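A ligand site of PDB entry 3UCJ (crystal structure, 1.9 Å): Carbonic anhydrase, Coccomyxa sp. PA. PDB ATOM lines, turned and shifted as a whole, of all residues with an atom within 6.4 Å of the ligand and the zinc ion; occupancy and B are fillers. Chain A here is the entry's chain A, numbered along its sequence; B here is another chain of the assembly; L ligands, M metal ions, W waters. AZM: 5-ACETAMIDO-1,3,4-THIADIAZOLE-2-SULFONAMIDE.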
ATOM      1  N   CYS A  47      32.228   5.238   5.827  1.00  0.00           N
ATOM      2  CA  CYS A  47      31.287   5.885   6.768  1.00  0.00           C
ATOM      3  C   CYS A  47      30.035   6.423   6.068  1.00  0.00           C
ATOM      4  O   CYS A  47      30.156   6.886   4.906  1.00  0.00           O
ATOM      5  CB  CYS A  47      32.028   7.048   7.527  1.00  0.00           C
ATOM      6  SG  CYS A  47      30.943   7.549   8.848  1.00  0.00           S
ATOM      7  N   ALA A  48      28.870   6.444   6.742  1.00  0.00           N
ATOM      8  CA  ALA A  48      27.653   6.907   6.240  1.00  0.00           C
ATOM      9  C   ALA A  48      27.644   8.478   6.108  1.00  0.00           C
ATOM     10  O   ALA A  48      26.791   9.012   5.502  1.00  0.00           O
ATOM     11  CB  ALA A  48      26.489   6.447   7.168  1.00  0.00           C
ATOM     12  N   ASP A  49      28.651   9.131   6.677  1.00  0.00           N
ATOM     13  CA  ASP A  49      28.818  10.619   6.630  1.00  0.00           C
ATOM     14  C   ASP A  49      28.563  11.160   5.211  1.00  0.00           C
ATOM     15  O   ASP A  49      29.144  10.664   4.250  1.00  0.00           O
ATOM     16  CB  ASP A  49      30.267  10.897   7.024  1.00  0.00           C
ATOM     17  CG  ASP A  49      30.530  12.418   7.267  1.00  0.00           C
ATOM     18  OD1 ASP A  49      30.332  13.203   6.324  1.00  0.00           O
ATOM     19  OD2 ASP A  49      30.812  12.780   8.426  1.00  0.00           O
ATOM     20  N   SER A  50      27.654  12.114   5.124  1.00  0.00           N
ATOM     21  CA  SER A  50      27.197  12.748   3.884  1.00  0.00           C
ATOM     22  C   SER A  50      28.301  13.403   3.058  1.00  0.00           C
ATOM     23  O   SER A  50      28.028  13.772   1.909  1.00  0.00           O
ATOM     24  CB  SER A  50      26.119  13.812   4.194  1.00  0.00           C
ATOM     25  OG  SER A  50      26.685  14.905   4.922  1.00  0.00           O
ATOM     26  N   ARG A  51      29.509  13.525   3.613  1.00  0.00           N
ATOM     27  CA  ARG A  51      30.573  14.201   2.891  1.00  0.00           C
ATOM     28  C   ARG A  51      31.456  13.246   2.126  1.00  0.00           C
ATOM     29  O   ARG A  51      32.467  13.677   1.493  1.00  0.00           O
ATOM     30  CB  ARG A  51      31.387  15.034   3.860  1.00  0.00           C
ATOM     31  CG  ARG A  51      30.558  16.125   4.393  1.00  0.00           C
ATOM     32  CD  ARG A  51      31.258  16.754   5.618  1.00  0.00           C
ATOM     33  NE  ARG A  51      31.444  15.814   6.755  1.00  0.00           N
ATOM     34  CZ  ARG A  51      32.225  16.060   7.809  1.00  0.00           C
ATOM     35  NH1 ARG A  51      32.966  17.204   7.888  1.00  0.00           N
ATOM     36  NH2 ARG A  51      32.352  15.117   8.753  1.00  0.00           N
ATOM     37  N   VAL A  52      31.123  11.950   2.214  1.00  0.00           N
ATOM     38  CA  VAL A  52      32.076  10.927   1.779  1.00  0.00           C
ATOM     39  C   VAL A  52      31.421   9.910   0.805  1.00  0.00           C
ATOM     40  O   VAL A  52      30.970   8.809   1.239  1.00  0.00           O
ATOM     41  CB  VAL A  52      32.689  10.136   2.974  1.00  0.00           C
ATOM     42  CG1 VAL A  52      33.917   9.304   2.534  1.00  0.00           C
ATOM     43  CG2 VAL A  52      33.035  11.126   4.168  1.00  0.00           C
ATOM     44  N   ASN A  70      28.251   2.624   6.875  1.00  0.00           N
ATOM     45  CA  ASN A  70      27.549   2.654   8.192  1.00  0.00           C
ATOM     46  C   ASN A  70      28.234   3.694   9.071  1.00  0.00           C
ATOM     47  O   ASN A  70      29.291   4.228   8.701  1.00  0.00           O
ATOM     48  CB  ASN A  70      27.595   1.224   8.832  1.00  0.00           C
ATOM     49  CG  ASN A  70      29.031   0.776   9.180  1.00  0.00           C
ATOM     50  OD1 ASN A  70      29.767   1.402   9.967  1.00  0.00           O
ATOM     51  ND2 ASN A  70      29.424  -0.383   8.638  1.00  0.00           N
ATOM     52  N   VAL A  71      27.631   3.998  10.207  1.00  0.00           N
ATOM     53  CA  VAL A  71      28.261   5.010  11.106  1.00  0.00           C
ATOM     54  C   VAL A  71      29.589   4.559  11.671  1.00  0.00           C
ATOM     55  O   VAL A  71      29.705   3.557  12.431  1.00  0.00           O
ATOM     56  CB  VAL A  71      27.213   5.371  12.270  1.00  0.00           C
ATOM     57  CG1 VAL A  71      27.983   6.069  13.437  1.00  0.00           C
ATOM     58  CG2 VAL A  71      25.989   6.106  11.696  1.00  0.00           C
ATOM     59  N   GLY A  72      30.667   5.285  11.312  1.00  0.00           N
ATOM     60  CA  GLY A  72      31.983   4.854  11.735  1.00  0.00           C
ATOM     61  C   GLY A  72      32.700   3.777  10.913  1.00  0.00           C
ATOM     62  O   GLY A  72      33.736   3.369  11.314  1.00  0.00           O
ATOM     63  N   ASN A  73      32.156   3.291   9.773  1.00  0.00           N
ATOM     64  CA  ASN A  73      32.866   2.363   8.955  1.00  0.00           C
ATOM     65  C   ASN A  73      33.377   1.148   9.712  1.00  0.00           C
ATOM     66  O   ASN A  73      34.518   0.731   9.632  1.00  0.00           O
ATOM     67  CB  ASN A  73      33.955   3.043   8.044  1.00  0.00           C
ATOM     68  CG  ASN A  73      35.008   3.871   8.796  1.00  0.00           C
ATOM     69  OD1 ASN A  73      34.891   5.125   8.876  1.00  0.00           O
ATOM     70  ND2 ASN A  73      36.068   3.233   9.217  1.00  0.00           N
ATOM     71  N   HIS A 103      37.469   8.384   7.678  1.00  0.00           N
ATOM     72  CA  HIS A 103      37.629   9.793   7.238  1.00  0.00           C
ATOM     73  C   HIS A 103      37.906  10.729   8.442  1.00  0.00           C
ATOM     74  O   HIS A 103      37.355  10.569   9.546  1.00  0.00           O
ATOM     75  CB  HIS A 103      36.395  10.279   6.479  1.00  0.00           C
ATOM     76  CG  HIS A 103      35.184  10.439   7.344  1.00  0.00           C
ATOM     77  ND1 HIS A 103      34.743  11.648   7.850  1.00  0.00           N
ATOM     78  CD2 HIS A 103      34.308   9.505   7.802  1.00  0.00           C
ATOM     79  CE1 HIS A 103      33.622  11.453   8.547  1.00  0.00           C
ATOM     80  NE2 HIS A 103      33.344  10.163   8.527  1.00  0.00           N
ATOM     81  N   ASN A 105      37.520  14.079  10.759  1.00  0.00           N
ATOM     82  CA  ASN A 105      36.312  14.787  11.127  1.00  0.00           C
ATOM     83  C   ASN A 105      35.078  13.830  11.251  1.00  0.00           C
ATOM     84  O   ASN A 105      33.928  14.245  11.088  1.00  0.00           O
ATOM     85  CB  ASN A 105      35.998  16.045  10.216  1.00  0.00           C
ATOM     86  CG  ASN A 105      35.107  17.052  10.914  1.00  0.00           C
ATOM     87  OD1 ASN A 105      33.946  17.297  10.514  1.00  0.00           O
ATOM     88  ND2 ASN A 105      35.675  17.753  11.938  1.00  0.00           N
ATOM     89  N   CYS A 106      35.353  12.576  11.587  1.00  0.00           N
ATOM     90  CA  CYS A 106      34.314  11.529  11.711  1.00  0.00           C
ATOM     91  C   CYS A 106      33.753  11.655  13.109  1.00  0.00           C
ATOM     92  O   CYS A 106      34.435  11.312  14.062  1.00  0.00           O
ATOM     93  CB  CYS A 106      34.968  10.158  11.522  1.00  0.00           C
ATOM     94  SG  CYS A 106      33.644   8.817  11.756  1.00  0.00           S
ATOM     95  N   GLY A 107      32.565  12.180  13.185  1.00  0.00           N
ATOM     96  CA  GLY A 107      31.855  12.307  14.410  1.00  0.00           C
ATOM     97  C   GLY A 107      31.621  11.003  15.143  1.00  0.00           C
ATOM     98  O   GLY A 107      31.480  11.031  16.386  1.00  0.00           O
ATOM     99  N   ALA A 108      31.622   9.875  14.432  1.00  0.00           N
ATOM    100  CA  ALA A 108      31.439   8.619  15.167  1.00  0.00           C
ATOM    101  C   ALA A 108      32.677   8.348  15.958  1.00  0.00           C
ATOM    102  O   ALA A 108      32.616   7.830  17.080  1.00  0.00           O
ATOM    103  CB  ALA A 108      31.154   7.392  14.146  1.00  0.00           C
ATOM    104  N   CYS A 109      33.862   8.636  15.376  1.00  0.00           N
ATOM    105  CA  CYS A 109      35.097   8.428  16.086  1.00  0.00           C
ATOM    106  C   CYS A 109      35.235   9.388  17.262  1.00  0.00           C
ATOM    107  O   CYS A 109      35.782   9.013  18.298  1.00  0.00           O
ATOM    108  CB  CYS A 109      36.331   8.622  15.194  1.00  0.00           C
ATOM    109  SG  CYS A 109      36.455   7.127  14.060  1.00  0.00           S
ATOM    110  N   ALA A 111      32.655  10.741  19.002  1.00  0.00           N
ATOM    111  CA  ALA A 111      31.732  10.241  20.017  1.00  0.00           C
ATOM    112  C   ALA A 111      32.340   9.012  20.734  1.00  0.00           C
ATOM    113  O   ALA A 111      32.243   8.884  21.941  1.00  0.00           O
ATOM    114  CB  ALA A 111      30.366   9.923  19.386  1.00  0.00           C
ATOM    115  N   TRP A 115      32.020  10.139  24.429  1.00  0.00           N
ATOM    116  CA  TRP A 115      30.748   9.879  25.090  1.00  0.00           C
ATOM    117  C   TRP A 115      30.953   8.975  26.317  1.00  0.00           C
ATOM    118  O   TRP A 115      31.790   8.003  26.295  1.00  0.00           O
ATOM    119  CB  TRP A 115      29.735   9.184  24.168  1.00  0.00           C
ATOM    120  CG  TRP A 115      29.032  10.102  23.194  1.00  0.00           C
ATOM    121  CD1 TRP A 115      29.355  11.455  22.910  1.00  0.00           C
ATOM    122  CD2 TRP A 115      27.874   9.822  22.425  1.00  0.00           C
ATOM    123  NE1 TRP A 115      28.479  11.949  21.977  1.00  0.00           N
ATOM    124  CE2 TRP A 115      27.555  10.989  21.670  1.00  0.00           C
ATOM    125  CE3 TRP A 115      27.049   8.677  22.293  1.00  0.00           C
ATOM    126  CZ2 TRP A 115      26.432  11.035  20.802  1.00  0.00           C
ATOM    127  CZ3 TRP A 115      25.987   8.712  21.452  1.00  0.00           C
ATOM    128  CH2 TRP A 115      25.649   9.871  20.724  1.00  0.00           C
ATOM    129  N   THR A 123      22.714   4.596  18.596  1.00  0.00           N
ATOM    130  CA  THR A 123      23.986   4.945  18.085  1.00  0.00           C
ATOM    131  C   THR A 123      25.086   4.678  19.118  1.00  0.00           C
ATOM    132  O   THR A 123      26.195   4.236  18.789  1.00  0.00           O
ATOM    133  CB  THR A 123      24.034   6.457  17.676  1.00  0.00           C
ATOM    134  OG1 THR A 123      22.983   6.719  16.748  1.00  0.00           O
ATOM    135  CG2 THR A 123      25.353   6.798  17.020  1.00  0.00           C
ATOM    136  N   ASN A 124      24.791   4.980  20.380  1.00  0.00           N
ATOM    137  CA  ASN A 124      25.769   4.749  21.417  1.00  0.00           C
ATOM    138  C   ASN A 124      26.098   3.171  21.505  1.00  0.00           C
ATOM    139  O   ASN A 124      27.225   2.789  21.711  1.00  0.00           O
ATOM    140  CB  ASN A 124      25.250   5.208  22.817  1.00  0.00           C
ATOM    141  CG  ASN A 124      26.310   4.917  23.887  1.00  0.00           C
ATOM    142  OD1 ASN A 124      27.461   5.408  23.838  1.00  0.00           O
ATOM    143  ND2 ASN A 124      25.967   4.055  24.808  1.00  0.00           N
ATOM    144  N   ILE A 127      28.459   2.381  18.338  1.00  0.00           N
ATOM    145  CA  ILE A 127      29.843   2.709  18.365  1.00  0.00           C
ATOM    146  C   ILE A 127      30.628   2.074  19.491  1.00  0.00           C
ATOM    147  O   ILE A 127      31.802   2.416  19.675  1.00  0.00           O
ATOM    148  CB  ILE A 127      29.982   4.352  18.419  1.00  0.00           C
ATOM    149  CG1 ILE A 127      29.434   4.802  19.787  1.00  0.00           C
ATOM    150  CG2 ILE A 127      29.275   4.923  17.182  1.00  0.00           C
ATOM    151  CD1 ILE A 127      29.770   6.386  20.022  1.00  0.00           C
ATOM    152  N   GLN B  38      28.576  18.889   8.794  1.00  0.00           N
ATOM    153  CA  GLN B  38      27.679  18.495   7.687  1.00  0.00           C
ATOM    154  C   GLN B  38      26.314  18.877   8.104  1.00  0.00           C
ATOM    155  O   GLN B  38      25.959  18.818   9.288  1.00  0.00           O
ATOM    156  CB  GLN B  38      27.720  16.961   7.397  1.00  0.00           C
ATOM    157  CG  GLN B  38      27.239  16.111   8.668  1.00  0.00           C
ATOM    158  CD  GLN B  38      27.442  14.573   8.460  1.00  0.00           C
ATOM    159  OE1 GLN B  38      27.130  14.012   7.374  1.00  0.00           O
ATOM    160  NE2 GLN B  38      27.904  13.897   9.497  1.00  0.00           N
ATOM    161  N   PHE B  66      23.292  11.777   3.495  1.00  0.00           N
ATOM    162  CA  PHE B  66      23.871  10.798   4.400  1.00  0.00           C
ATOM    163  C   PHE B  66      23.346   9.416   3.896  1.00  0.00           C
ATOM    164  O   PHE B  66      22.189   9.320   3.534  1.00  0.00           O
ATOM    165  CB  PHE B  66      23.253  11.091   5.769  1.00  0.00           C
ATOM    166  CG  PHE B  66      23.995  10.466   6.919  1.00  0.00           C
ATOM    167  CD1 PHE B  66      24.936  11.214   7.653  1.00  0.00           C
ATOM    168  CD2 PHE B  66      23.673   9.166   7.379  1.00  0.00           C
ATOM    169  CE1 PHE B  66      25.573  10.690   8.751  1.00  0.00           C
ATOM    170  CE2 PHE B  66      24.361   8.601   8.515  1.00  0.00           C
ATOM    171  CZ  PHE B  66      25.311   9.333   9.184  1.00  0.00           C
ATOM    172  N   TYR B  88      20.982   8.823  14.109  1.00  0.00           N
ATOM    173  CA  TYR B  88      21.847   9.983  14.003  1.00  0.00           C
ATOM    174  C   TYR B  88      21.328  11.083  13.079  1.00  0.00           C
ATOM    175  O   TYR B  88      21.455  12.228  13.392  1.00  0.00           O
ATOM    176  CB  TYR B  88      23.281   9.626  13.646  1.00  0.00           C
ATOM    177  CG  TYR B  88      24.183  10.823  13.669  1.00  0.00           C
ATOM    178  CD1 TYR B  88      24.434  11.519  14.837  1.00  0.00           C
ATOM    179  CD2 TYR B  88      24.759  11.295  12.521  1.00  0.00           C
ATOM    180  CE1 TYR B  88      25.221  12.606  14.846  1.00  0.00           C
ATOM    181  CE2 TYR B  88      25.547  12.381  12.530  1.00  0.00           C
ATOM    182  CZ  TYR B  88      25.777  13.054  13.679  1.00  0.00           C
ATOM    183  OH  TYR B  88      26.564  14.162  13.683  1.00  0.00           O
ATOM    184  N   HIS B  92      19.928  13.952  15.462  1.00  0.00           N
ATOM    185  CA  HIS B  92      20.990  14.872  15.658  1.00  0.00           C
ATOM    186  C   HIS B  92      21.126  15.799  14.435  1.00  0.00           C
ATOM    187  O   HIS B  92      21.120  16.979  14.600  1.00  0.00           O
ATOM    188  CB  HIS B  92      22.280  14.113  15.895  1.00  0.00           C
ATOM    189  CG  HIS B  92      22.381  13.408  17.219  1.00  0.00           C
ATOM    190  ND1 HIS B  92      23.276  13.807  18.198  1.00  0.00           N
ATOM    191  CD2 HIS B  92      21.794  12.282  17.686  1.00  0.00           C
ATOM    192  CE1 HIS B  92      23.219  12.963  19.216  1.00  0.00           C
ATOM    193  NE2 HIS B  92      22.325  12.034  18.937  1.00  0.00           N
ATOM    194  N   LEU B  93      21.223  15.255  13.231  1.00  0.00           N
ATOM    195  CA  LEU B  93      21.306  16.148  12.078  1.00  0.00           C
ATOM    196  C   LEU B  93      20.012  16.801  11.675  1.00  0.00           C
ATOM    197  O   LEU B  93      20.060  17.763  10.930  1.00  0.00           O
ATOM    198  CB  LEU B  93      21.931  15.458  10.856  1.00  0.00           C
ATOM    199  CG  LEU B  93      23.300  14.862  11.021  1.00  0.00           C
ATOM    200  CD1 LEU B  93      23.722  14.095   9.721  1.00  0.00           C
ATOM    201  CD2 LEU B  93      24.385  15.859  11.398  1.00  0.00           C
HETATM  202  C1  AZM L   1      28.941  10.966  12.622  1.00  0.00           C
HETATM  203  C2  AZM L   1      28.249  11.133  14.929  1.00  0.00           C
HETATM  204  C3  AZM L   1      27.526   9.945  16.867  1.00  0.00           C
HETATM  205  C4  AZM L   1      26.788  10.006  18.183  1.00  0.00           C
HETATM  206  N1  AZM L   1      30.837  10.603  10.630  1.00  0.00           N
HETATM  207  N2  AZM L   1      28.758  12.309  14.422  1.00  0.00           N
HETATM  208  N3  AZM L   1      29.181  12.228  12.992  1.00  0.00           N
HETATM  209  N4  AZM L   1      27.954  11.086  16.320  1.00  0.00           N
HETATM  210  O1  AZM L   1      28.436  10.966  10.062  1.00  0.00           O
HETATM  211  O2  AZM L   1      29.208   8.990  11.194  1.00  0.00           O
HETATM  212  O3  AZM L   1      27.745   8.855  16.261  1.00  0.00           O
HETATM  213  S1  AZM L   1      29.305  10.475  10.988  1.00  0.00           S
HETATM  214  S2  AZM L   1      28.185   9.873  13.800  1.00  0.00           S
HETATM  215 ZN    ZN M   1      32.101   9.293   9.956  1.00  0.00          ZN
HETATM  216  O   HOH W   1      27.937  13.417  17.661  1.00  0.00           O
HETATM  217  O   HOH W   2      29.249  14.565  15.641  1.00  0.00           O
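The side-chain amide nitrogen (NE2) of Gln 38 of chain B sits at hydrogen-bond distance from the side-chain carboxylate (OD2) of Asp 49, at 3.3 Å. The side-chain amide oxygen (OE1) of Gln 38 of chain B sits at hydrogen-bond distance from the side-chain hydroxyl (OG) of Ser 50, 2.6 Å away. The side-chain sulfur of Cys 47 sits close to the backbone carbonyl oxygen of Asn 70. SG of Cys 106 lies close to N of Cys 109 (3.6 Å). N of Ala 108 sits close to SG of Cys 106 (3.5 Å). The backbone NH (N) of Asp 49 lies close to the side-chain sulfur (SG) of Cys 47 (3.5 Å). SG of Cys 47 lies close to N of Gly 72 (3.4 Å). The side-chain carboxylate (OD2) of Asp 49 lies within salt-bridge range of the guanidinium group (NH2) of Arg 51 (2.8 Å).
A nitrogen (N2) of the ligand sits at hydrogen-bond distance from the side-chain hydroxyl (OH) of Tyr 88 of chain B (3.0 Å). The side-chain carboxylate (OD2) of Asp 49 lies close to a nitrogen (N1) of the ligand (3.1 Å). The backbone NH (N) of Ala 108 lies close to a sulfur (S2) of the ligand. An oxygen (O1) of the ligand is in hydrogen-bond range of the side-chain amide nitrogen (NE2) of Gln 38 of chain B (3.0 Å). N of Gly 107 sits close to N3 of the ligand (3.4 Å).
CG1 of Val 71 touches S2 of the ligand, at 3.8 Å. Gly 72 touches the ligand. CB of Ala 111 touches C4 of the ligand (3.8 Å). Trp 115 touches the ligand (CH2 to C4, 2.8 Å). CG2 of Thr 123 touches O3 of the ligand, 3.2 Å away. Phe 66 of chain B touches the ligand (CE1 to O1, 3.2 Å). Hydrophobic or aromatic side chains within 4 Å of the ligand: Val 71, His 103, Ala 108, Ala 111, Trp 115, Phe 66 of chain B and Tyr 88 of chain B. Within 4 Å of the ligand: Cys 47, Asp 49, Val 71, Gly 72, His 103, Cys 106, Gly 107, Ala 108, Ala 111, Trp 115, Thr 123, Gln 38 of chain B, Phe 66 of chain B and Tyr 88 of chain B. The nearest printed residue that does not touch the ligand is Ile 127 (4.3 Å).
Water W2 bridges a nitrogen (N2) of the ligand (2.6 Å) and the side-chain hydroxyl of Tyr 88 of chain B (3.3 Å).
Residues that only touch the zinc ion: Asp 49. Along chain A the residues within 4 Å of the zinc ion span positions 47 to 106.
The zinc ion is bound by a nitrogen (N1) of the ligand (1.9 Å). NE2 of His 103 binds the zinc ion (2.1 Å). SG of Cys 47 binds the zinc ion (2.4 Å). The zinc ion is bound by the side-chain sulfur (SG) of Cys 106 (2.4 Å).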
